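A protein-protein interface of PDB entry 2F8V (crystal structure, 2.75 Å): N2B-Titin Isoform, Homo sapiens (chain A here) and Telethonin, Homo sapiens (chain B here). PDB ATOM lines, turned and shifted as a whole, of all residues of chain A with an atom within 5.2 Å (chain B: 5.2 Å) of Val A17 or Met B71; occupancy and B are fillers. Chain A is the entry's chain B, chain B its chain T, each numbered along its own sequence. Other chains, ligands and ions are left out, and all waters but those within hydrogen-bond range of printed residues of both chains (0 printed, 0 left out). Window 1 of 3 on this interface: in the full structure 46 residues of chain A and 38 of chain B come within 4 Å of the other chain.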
ATOM      1  N   VAL A  15      30.267  27.835 -31.723  1.00  0.00           N
ATOM      2  CA  VAL A  15      30.038  27.558 -30.311  1.00  0.00           C
ATOM      3  C   VAL A  15      28.818  28.271 -29.740  1.00  0.00           C
ATOM      4  O   VAL A  15      28.520  29.432 -30.076  1.00  0.00           O
ATOM      5  CB  VAL A  15      31.287  27.877 -29.416  1.00  0.00           C
ATOM      6  CG1 VAL A  15      32.512  27.115 -29.869  1.00  0.00           C
ATOM      7  CG2 VAL A  15      31.563  29.340 -29.371  1.00  0.00           C
ATOM      8  N   VAL A  16      28.122  27.570 -28.850  1.00  0.00           N
ATOM      9  CA  VAL A  16      27.010  28.163 -28.115  1.00  0.00           C
ATOM     10  C   VAL A  16      27.429  28.348 -26.688  1.00  0.00           C
ATOM     11  O   VAL A  16      27.894  27.403 -26.058  1.00  0.00           O
ATOM     12  CB  VAL A  16      25.788  27.242 -28.093  1.00  0.00           C
ATOM     13  CG1 VAL A  16      24.537  28.069 -27.887  1.00  0.00           C
ATOM     14  CG2 VAL A  16      25.699  26.497 -29.400  1.00  0.00           C
ATOM     15  N   VAL A  17      27.263  29.555 -26.166  1.00  0.00           N
ATOM     16  CA  VAL A  17      27.617  29.787 -24.770  1.00  0.00           C
ATOM     17  C   VAL A  17      26.600  30.655 -24.009  1.00  0.00           C
ATOM     18  O   VAL A  17      25.693  31.300 -24.598  1.00  0.00           O
ATOM     19  CB  VAL A  17      29.026  30.383 -24.651  1.00  0.00           C
ATOM     20  CG1 VAL A  17      30.038  29.409 -25.185  1.00  0.00           C
ATOM     21  CG2 VAL A  17      29.106  31.647 -25.434  1.00  0.00           C
ATOM     22  N   LEU A  18      26.772  30.660 -22.690  1.00  0.00           N
ATOM     23  CA  LEU A  18      25.870  31.361 -21.790  1.00  0.00           C
ATOM     24  C   LEU A  18      26.303  32.809 -21.637  1.00  0.00           C
ATOM     25  O   LEU A  18      27.417  33.105 -21.212  1.00  0.00           O
ATOM     26  CB  LEU A  18      25.860  30.664 -20.430  1.00  0.00           C
ATOM     27  CG  LEU A  18      24.633  30.867 -19.542  1.00  0.00           C
ATOM     28  CD1 LEU A  18      25.028  30.789 -18.077  1.00  0.00           C
ATOM     29  CD2 LEU A  18      23.996  32.219 -19.866  1.00  0.00           C
ATOM     30  N   GLU A  19      25.426  33.722 -22.009  1.00  0.00           N
ATOM     31  CA  GLU A  19      25.706  35.131 -21.777  1.00  0.00           C
ATOM     32  C   GLU A  19      26.424  35.238 -20.430  1.00  0.00           C
ATOM     33  O   GLU A  19      25.986  34.640 -19.455  1.00  0.00           O
ATOM     34  CB  GLU A  19      24.394  35.927 -21.743  1.00  0.00           C
ATOM     35  CG  GLU A  19      24.555  37.345 -21.286  1.00  0.00           C
ATOM     36  CD  GLU A  19      23.361  38.210 -21.660  1.00  0.00           C
ATOM     37  OE1 GLU A  19      22.224  37.863 -21.268  1.00  0.00           O
ATOM     38  OE2 GLU A  19      23.555  39.245 -22.343  1.00  0.00           O
ATOM     39  N   SER A  21      29.503  34.130 -19.762  1.00  0.00           N
ATOM     40  CA  SER A  21      30.654  33.232 -19.677  1.00  0.00           C
ATOM     41  C   SER A  21      31.686  33.444 -20.791  1.00  0.00           C
ATOM     42  O   SER A  21      31.529  34.332 -21.657  1.00  0.00           O
ATOM     43  CB  SER A  21      30.188  31.799 -19.669  1.00  0.00           C
ATOM     44  OG  SER A  21      29.430  31.579 -20.808  1.00  0.00           O
ATOM     45  N   THR A  22      32.740  32.626 -20.758  1.00  0.00           N
ATOM     46  CA  THR A  22      33.860  32.746 -21.684  1.00  0.00           C
ATOM     47  C   THR A  22      33.610  31.963 -22.970  1.00  0.00           C
ATOM     48  O   THR A  22      33.001  30.898 -22.932  1.00  0.00           O
ATOM     49  CB  THR A  22      35.166  32.234 -21.002  1.00  0.00           C
ATOM     50  OG1 THR A  22      36.304  32.903 -21.559  1.00  0.00           O
ATOM     51  CG2 THR A  22      35.404  30.757 -21.322  1.00  0.00           C
ATOM     52  N   ALA A  23      34.067  32.486 -24.107  1.00  0.00           N
ATOM     53  CA  ALA A  23      33.969  31.759 -25.388  1.00  0.00           C
ATOM     54  C   ALA A  23      35.320  31.697 -26.031  1.00  0.00           C
ATOM     55  O   ALA A  23      36.090  32.649 -25.936  1.00  0.00           O
ATOM     56  CB  ALA A  23      32.996  32.438 -26.354  1.00  0.00           C
ATOM     57  N   VAL A  70      31.192  36.976 -22.422  1.00  0.00           N
ATOM     58  CA  VAL A  70      30.521  37.337 -23.657  1.00  0.00           C
ATOM     59  C   VAL A  70      29.199  38.018 -23.391  1.00  0.00           C
ATOM     60  O   VAL A  70      28.499  37.670 -22.453  1.00  0.00           O
ATOM     61  CB  VAL A  70      30.250  36.122 -24.521  1.00  0.00           C
ATOM     62  CG1 VAL A  70      31.539  35.411 -24.876  1.00  0.00           C
ATOM     63  CG2 VAL A  70      29.336  35.170 -23.770  1.00  0.00           C
ATOM     64  N   LEU A  95      29.299  32.370 -33.356  1.00  0.00           N
ATOM     65  CA  LEU A  95      29.262  32.464 -31.917  1.00  0.00           C
ATOM     66  C   LEU A  95      27.823  32.754 -31.589  1.00  0.00           C
ATOM     67  O   LEU A  95      27.289  33.777 -32.028  1.00  0.00           O
ATOM     68  CB  LEU A  95      30.106  33.637 -31.436  1.00  0.00           C
ATOM     69  CG  LEU A  95      29.890  33.980 -29.958  1.00  0.00           C
ATOM     70  CD1 LEU A  95      30.258  32.799 -29.071  1.00  0.00           C
ATOM     71  CD2 LEU A  95      30.658  35.259 -29.556  1.00  0.00           C
ATOM     72  N   LEU A  96      27.188  31.851 -30.840  1.00  0.00           N
ATOM     73  CA  LEU A  96      25.795  32.029 -30.446  1.00  0.00           C
ATOM     74  C   LEU A  96      25.667  32.181 -28.934  1.00  0.00           C
ATOM     75  O   LEU A  96      25.953  31.255 -28.164  1.00  0.00           O
ATOM     76  CB  LEU A  96      24.980  30.858 -30.930  1.00  0.00           C
ATOM     77  CG  LEU A  96      25.139  30.726 -32.427  1.00  0.00           C
ATOM     78  CD1 LEU A  96      25.541  29.313 -32.840  1.00  0.00           C
ATOM     79  CD2 LEU A  96      23.850  31.169 -33.110  1.00  0.00           C
ATOM     80  N   VAL A  97      25.249  33.368 -28.522  1.00  0.00           N
ATOM     81  CA  VAL A  97      25.139  33.737 -27.121  1.00  0.00           C
ATOM     82  C   VAL A  97      23.711  33.617 -26.607  1.00  0.00           C
ATOM     83  O   VAL A  97      22.813  34.347 -27.038  1.00  0.00           O
ATOM     84  CB  VAL A  97      25.539  35.178 -26.958  1.00  0.00           C
ATOM     85  CG1 VAL A  97      25.506  35.570 -25.491  1.00  0.00           C
ATOM     86  CG2 VAL A  97      26.878  35.403 -27.579  1.00  0.00           C
ATOM     87  N   LYS A  98      23.517  32.704 -25.668  1.00  0.00           N
ATOM     88  CA  LYS A  98      22.194  32.444 -25.114  1.00  0.00           C
ATOM     89  C   LYS A  98      22.022  33.064 -23.708  1.00  0.00           C
ATOM     90  O   LYS A  98      22.932  32.987 -22.861  1.00  0.00           O
ATOM     91  CB  LYS A  98      21.972  30.933 -25.061  1.00  0.00           C
ATOM     92  CG  LYS A  98      21.773  30.285 -26.430  1.00  0.00           C
ATOM     93  CD  LYS A  98      20.427  30.727 -27.025  1.00  0.00           C
ATOM     94  CE  LYS A  98      20.278  30.336 -28.490  1.00  0.00           C
ATOM     95  NZ  LYS A  98      19.004  30.919 -28.991  1.00  0.00           N
ATOM     96  N   LEU B  60      21.929  22.946 -29.808  1.00  0.00           N
ATOM     97  CA  LEU B  60      21.008  22.360 -28.847  1.00  0.00           C
ATOM     98  C   LEU B  60      21.063  23.080 -27.504  1.00  0.00           C
ATOM     99  O   LEU B  60      22.103  23.121 -26.850  1.00  0.00           O
ATOM    100  CB  LEU B  60      21.356  20.889 -28.693  1.00  0.00           C
ATOM    101  CG  LEU B  60      20.668  20.042 -27.633  1.00  0.00           C
ATOM    102  CD1 LEU B  60      20.739  18.560 -28.010  1.00  0.00           C
ATOM    103  CD2 LEU B  60      21.327  20.282 -26.292  1.00  0.00           C
ATOM    104  N   VAL B  61      19.949  23.669 -27.094  1.00  0.00           N
ATOM    105  CA  VAL B  61      19.895  24.411 -25.826  1.00  0.00           C
ATOM    106  C   VAL B  61      18.829  23.821 -24.956  1.00  0.00           C
ATOM    107  O   VAL B  61      17.666  23.799 -25.366  1.00  0.00           O
ATOM    108  CB  VAL B  61      19.471  25.834 -26.044  1.00  0.00           C
ATOM    109  CG1 VAL B  61      19.425  26.559 -24.733  1.00  0.00           C
ATOM    110  CG2 VAL B  61      20.410  26.517 -26.995  1.00  0.00           C
ATOM    111  N   GLN B  62      19.211  23.346 -23.768  1.00  0.00           N
ATOM    112  CA  GLN B  62      18.253  22.735 -22.862  1.00  0.00           C
ATOM    113  C   GLN B  62      18.120  23.502 -21.565  1.00  0.00           C
ATOM    114  O   GLN B  62      19.068  24.165 -21.143  1.00  0.00           O
ATOM    115  CB  GLN B  62      18.636  21.299 -22.579  1.00  0.00           C
ATOM    116  CG  GLN B  62      17.502  20.454 -22.019  1.00  0.00           C
ATOM    117  CD  GLN B  62      17.976  19.108 -21.492  1.00  0.00           C
ATOM    118  OE1 GLN B  62      17.196  18.156 -21.438  1.00  0.00           O
ATOM    119  NE2 GLN B  62      19.254  19.025 -21.085  1.00  0.00           N
ATOM    120  N   MET B  69      21.022  24.879 -16.950  1.00  0.00           N
ATOM    121  CA  MET B  69      20.922  24.862 -18.413  1.00  0.00           C
ATOM    122  C   MET B  69      21.957  23.934 -19.013  1.00  0.00           C
ATOM    123  O   MET B  69      22.908  23.515 -18.355  1.00  0.00           O
ATOM    124  CB  MET B  69      21.100  26.267 -18.997  1.00  0.00           C
ATOM    125  CG  MET B  69      19.976  27.232 -18.710  1.00  0.00           C
ATOM    126  SD  MET B  69      20.082  28.690 -19.754  1.00  0.00           S
ATOM    127  CE  MET B  69      18.993  28.299 -21.050  1.00  0.00           C
ATOM    128  N   ARG B  70      21.777  23.642 -20.288  1.00  0.00           N
ATOM    129  CA  ARG B  70      22.669  22.753 -21.014  1.00  0.00           C
ATOM    130  C   ARG B  70      22.702  23.224 -22.457  1.00  0.00           C
ATOM    131  O   ARG B  70      21.655  23.512 -23.053  1.00  0.00           O
ATOM    132  CB  ARG B  70      22.073  21.363 -20.975  1.00  0.00           C
ATOM    133  CG  ARG B  70      23.073  20.263 -21.134  1.00  0.00           C
ATOM    134  CD  ARG B  70      23.479  19.674 -19.811  1.00  0.00           C
ATOM    135  NE  ARG B  70      22.331  19.143 -19.079  1.00  0.00           N
ATOM    136  CZ  ARG B  70      21.901  17.899 -19.204  1.00  0.00           C
ATOM    137  NH1 ARG B  70      22.516  17.075 -20.041  1.00  0.00           N
ATOM    138  NH2 ARG B  70      20.861  17.474 -18.513  1.00  0.00           N
ATOM    139  N   MET B  71      23.873  23.310 -23.056  1.00  0.00           N
ATOM    140  CA  MET B  71      23.876  23.763 -24.437  1.00  0.00           C
ATOM    141  C   MET B  71      25.084  23.272 -25.220  1.00  0.00           C
ATOM    142  O   MET B  71      26.090  22.888 -24.631  1.00  0.00           O
ATOM    143  CB  MET B  71      23.730  25.295 -24.497  1.00  0.00           C
ATOM    144  CG  MET B  71      24.958  26.052 -24.066  1.00  0.00           C
ATOM    145  SD  MET B  71      24.670  27.828 -23.949  1.00  0.00           S
ATOM    146  CE  MET B  71      23.562  27.920 -22.523  1.00  0.00           C
ATOM    147  N   GLY B  72      24.964  23.277 -26.545  1.00  0.00           N
ATOM    148  CA  GLY B  72      26.050  22.858 -27.425  1.00  0.00           C
ATOM    149  C   GLY B  72      25.660  22.581 -28.867  1.00  0.00           C
ATOM    150  O   GLY B  72      24.484  22.699 -29.251  1.00  0.00           O
ATOM    151  N   ILE B  73      26.651  22.207 -29.666  1.00  0.00           N
ATOM    152  CA  ILE B  73      26.426  21.873 -31.065  1.00  0.00           C
ATOM    153  C   ILE B  73      26.322  20.387 -31.110  1.00  0.00           C
ATOM    154  O   ILE B  73      27.090  19.683 -30.452  1.00  0.00           O
ATOM    155  CB  ILE B  73      27.592  22.295 -31.933  1.00  0.00           C
ATOM    156  CG1 ILE B  73      27.868  23.780 -31.752  1.00  0.00           C
ATOM    157  CG2 ILE B  73      27.279  22.041 -33.389  1.00  0.00           C
ATOM    158  CD1 ILE B  73      26.901  24.655 -32.485  1.00  0.00           C
ATOM    159  N   GLY B  77      30.480  18.151 -27.624  1.00  0.00           N
ATOM    160  CA  GLY B  77      29.909  17.946 -26.315  1.00  0.00           C
ATOM    161  C   GLY B  77      28.943  19.035 -25.874  1.00  0.00           C
ATOM    162  O   GLY B  77      28.952  20.144 -26.399  1.00  0.00           O
ATOM    163  N   LEU B  78      28.110  18.701 -24.896  1.00  0.00           N
ATOM    164  CA  LEU B  78      27.288  19.676 -24.200  1.00  0.00           C
ATOM    165  C   LEU B  78      28.012  20.304 -23.000  1.00  0.00           C
ATOM    166  O   LEU B  78      28.865  19.679 -22.358  1.00  0.00           O
ATOM    167  CB  LEU B  78      26.012  19.013 -23.681  1.00  0.00           C
ATOM    168  CG  LEU B  78      25.033  18.375 -24.661  1.00  0.00           C
ATOM    169  CD1 LEU B  78      23.637  18.600 -24.117  1.00  0.00           C
ATOM    170  CD2 LEU B  78      25.165  19.002 -26.047  1.00  0.00           C
ATOM    171  N   GLN B  79      27.634  21.534 -22.686  1.00  0.00           N
ATOM    172  CA  GLN B  79      28.161  22.230 -21.538  1.00  0.00           C
ATOM    173  C   GLN B  79      27.032  22.424 -20.522  1.00  0.00           C
ATOM    174  O   GLN B  79      25.898  22.714 -20.897  1.00  0.00           O
ATOM    175  CB  GLN B  79      28.714  23.580 -21.993  1.00  0.00           C
ATOM    176  CG  GLN B  79      29.247  24.461 -20.884  1.00  0.00           C
ATOM    177  CD  GLN B  79      30.683  24.156 -20.529  1.00  0.00           C
ATOM    178  OE1 GLN B  79      31.461  23.755 -21.395  1.00  0.00           O
ATOM    179  NE2 GLN B  79      31.044  24.353 -19.266  1.00  0.00           N
ATOM    180  N   TYR B  81      25.580  24.520 -17.251  1.00  0.00           N
ATOM    181  CA  TYR B  81      25.714  25.708 -16.420  1.00  0.00           C
ATOM    182  C   TYR B  81      24.786  25.617 -15.218  1.00  0.00           C
ATOM    183  O   TYR B  81      23.773  24.945 -15.263  1.00  0.00           O
ATOM    184  CB  TYR B  81      25.382  26.959 -17.223  1.00  0.00           C
ATOM    185  CG  TYR B  81      26.291  27.236 -18.395  1.00  0.00           C
ATOM    186  CD1 TYR B  81      26.050  26.668 -19.649  1.00  0.00           C
ATOM    187  CD2 TYR B  81      27.355  28.096 -18.266  1.00  0.00           C
ATOM    188  CE1 TYR B  81      26.871  26.939 -20.719  1.00  0.00           C
ATOM    189  CE2 TYR B  81      28.172  28.372 -19.323  1.00  0.00           C
ATOM    190  CZ  TYR B  81      27.935  27.797 -20.537  1.00  0.00           C
ATOM    191  OH  TYR B  81      28.778  28.106 -21.571  1.00  0.00           O
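N of Tyr B81 lies within hydrogen-bond range of O of Met B69.
O of Val A17 lies within hydrogen-bond range of N of Lys A98, 2.8 Å away.
O of Gly B72 sits at hydrogen-bond distance from N of Leu B60 (2.6 Å).
The backbone carbonyl oxygen of Met B71 is in hydrogen-bond range of the backbone NH of Gln B79 (2.8 Å).
N of Val A17 lies within hydrogen-bond range of O of Leu A96, 2.9 Å away.
O of Ser A21 sits at hydrogen-bond distance from N of Val A70 (2.8 Å).
Val A17 touches two residues of chain B.
Of chain A, only Val A16 (3.8 Å), Val A17 (3.4 Å) and Leu A18 (3.7 Å) come within 4 Å of Met B71.
Of the printed residues of chain B, Leu A18 touches Met B71 (3.7 Å) and Tyr B81 (3.4 Å).
Printed residues of chain A within 4 Å of Tyr B81: Val A17, Leu A18 and Ser A21.
Of the printed residues of chain B, Val A16 touches Met B71, Gly B72 and Ile B73.
Of the printed residues of chain A, Ile B73 touches Val A16 (3.8 Å).
The nearest printed residue of chain B that does not touch Val A17 is Gln B79 (6.6 Å).
Among the printed residues, pairs that only touch across the chains: Val A16 with Met B71 (3.8 Å), Val A16 with Gly B72 (3.95 Å), Val A16 with Ile B73 (3.8 Å), Val A17 with Tyr B81 (3.8 Å) and Ser A21 with Tyr B81 (3.6 Å).
The backbone NH of Leu A18 is in hydrogen-bond range of the side-chain sulfur of Met B71, 3.7 Å away.
The side-chain sulfur (SD) of Met B71 sits close to the backbone carbonyl oxygen (O) of Val A17 (3.7 Å).
The side-chain hydroxyl (OH) of Tyr B81 lies within hydrogen-bond range of the backbone NH (N) of Leu A18 (3.4 Å).
Printed residues of chain A that touch a printed residue of chain B: Val A16, Val A17, Leu A18 and Ser A21.
Hydrophobic or aromatic side chains of chain A that line the printed part of chain B: Val A16, Val A17 and Leu A18.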
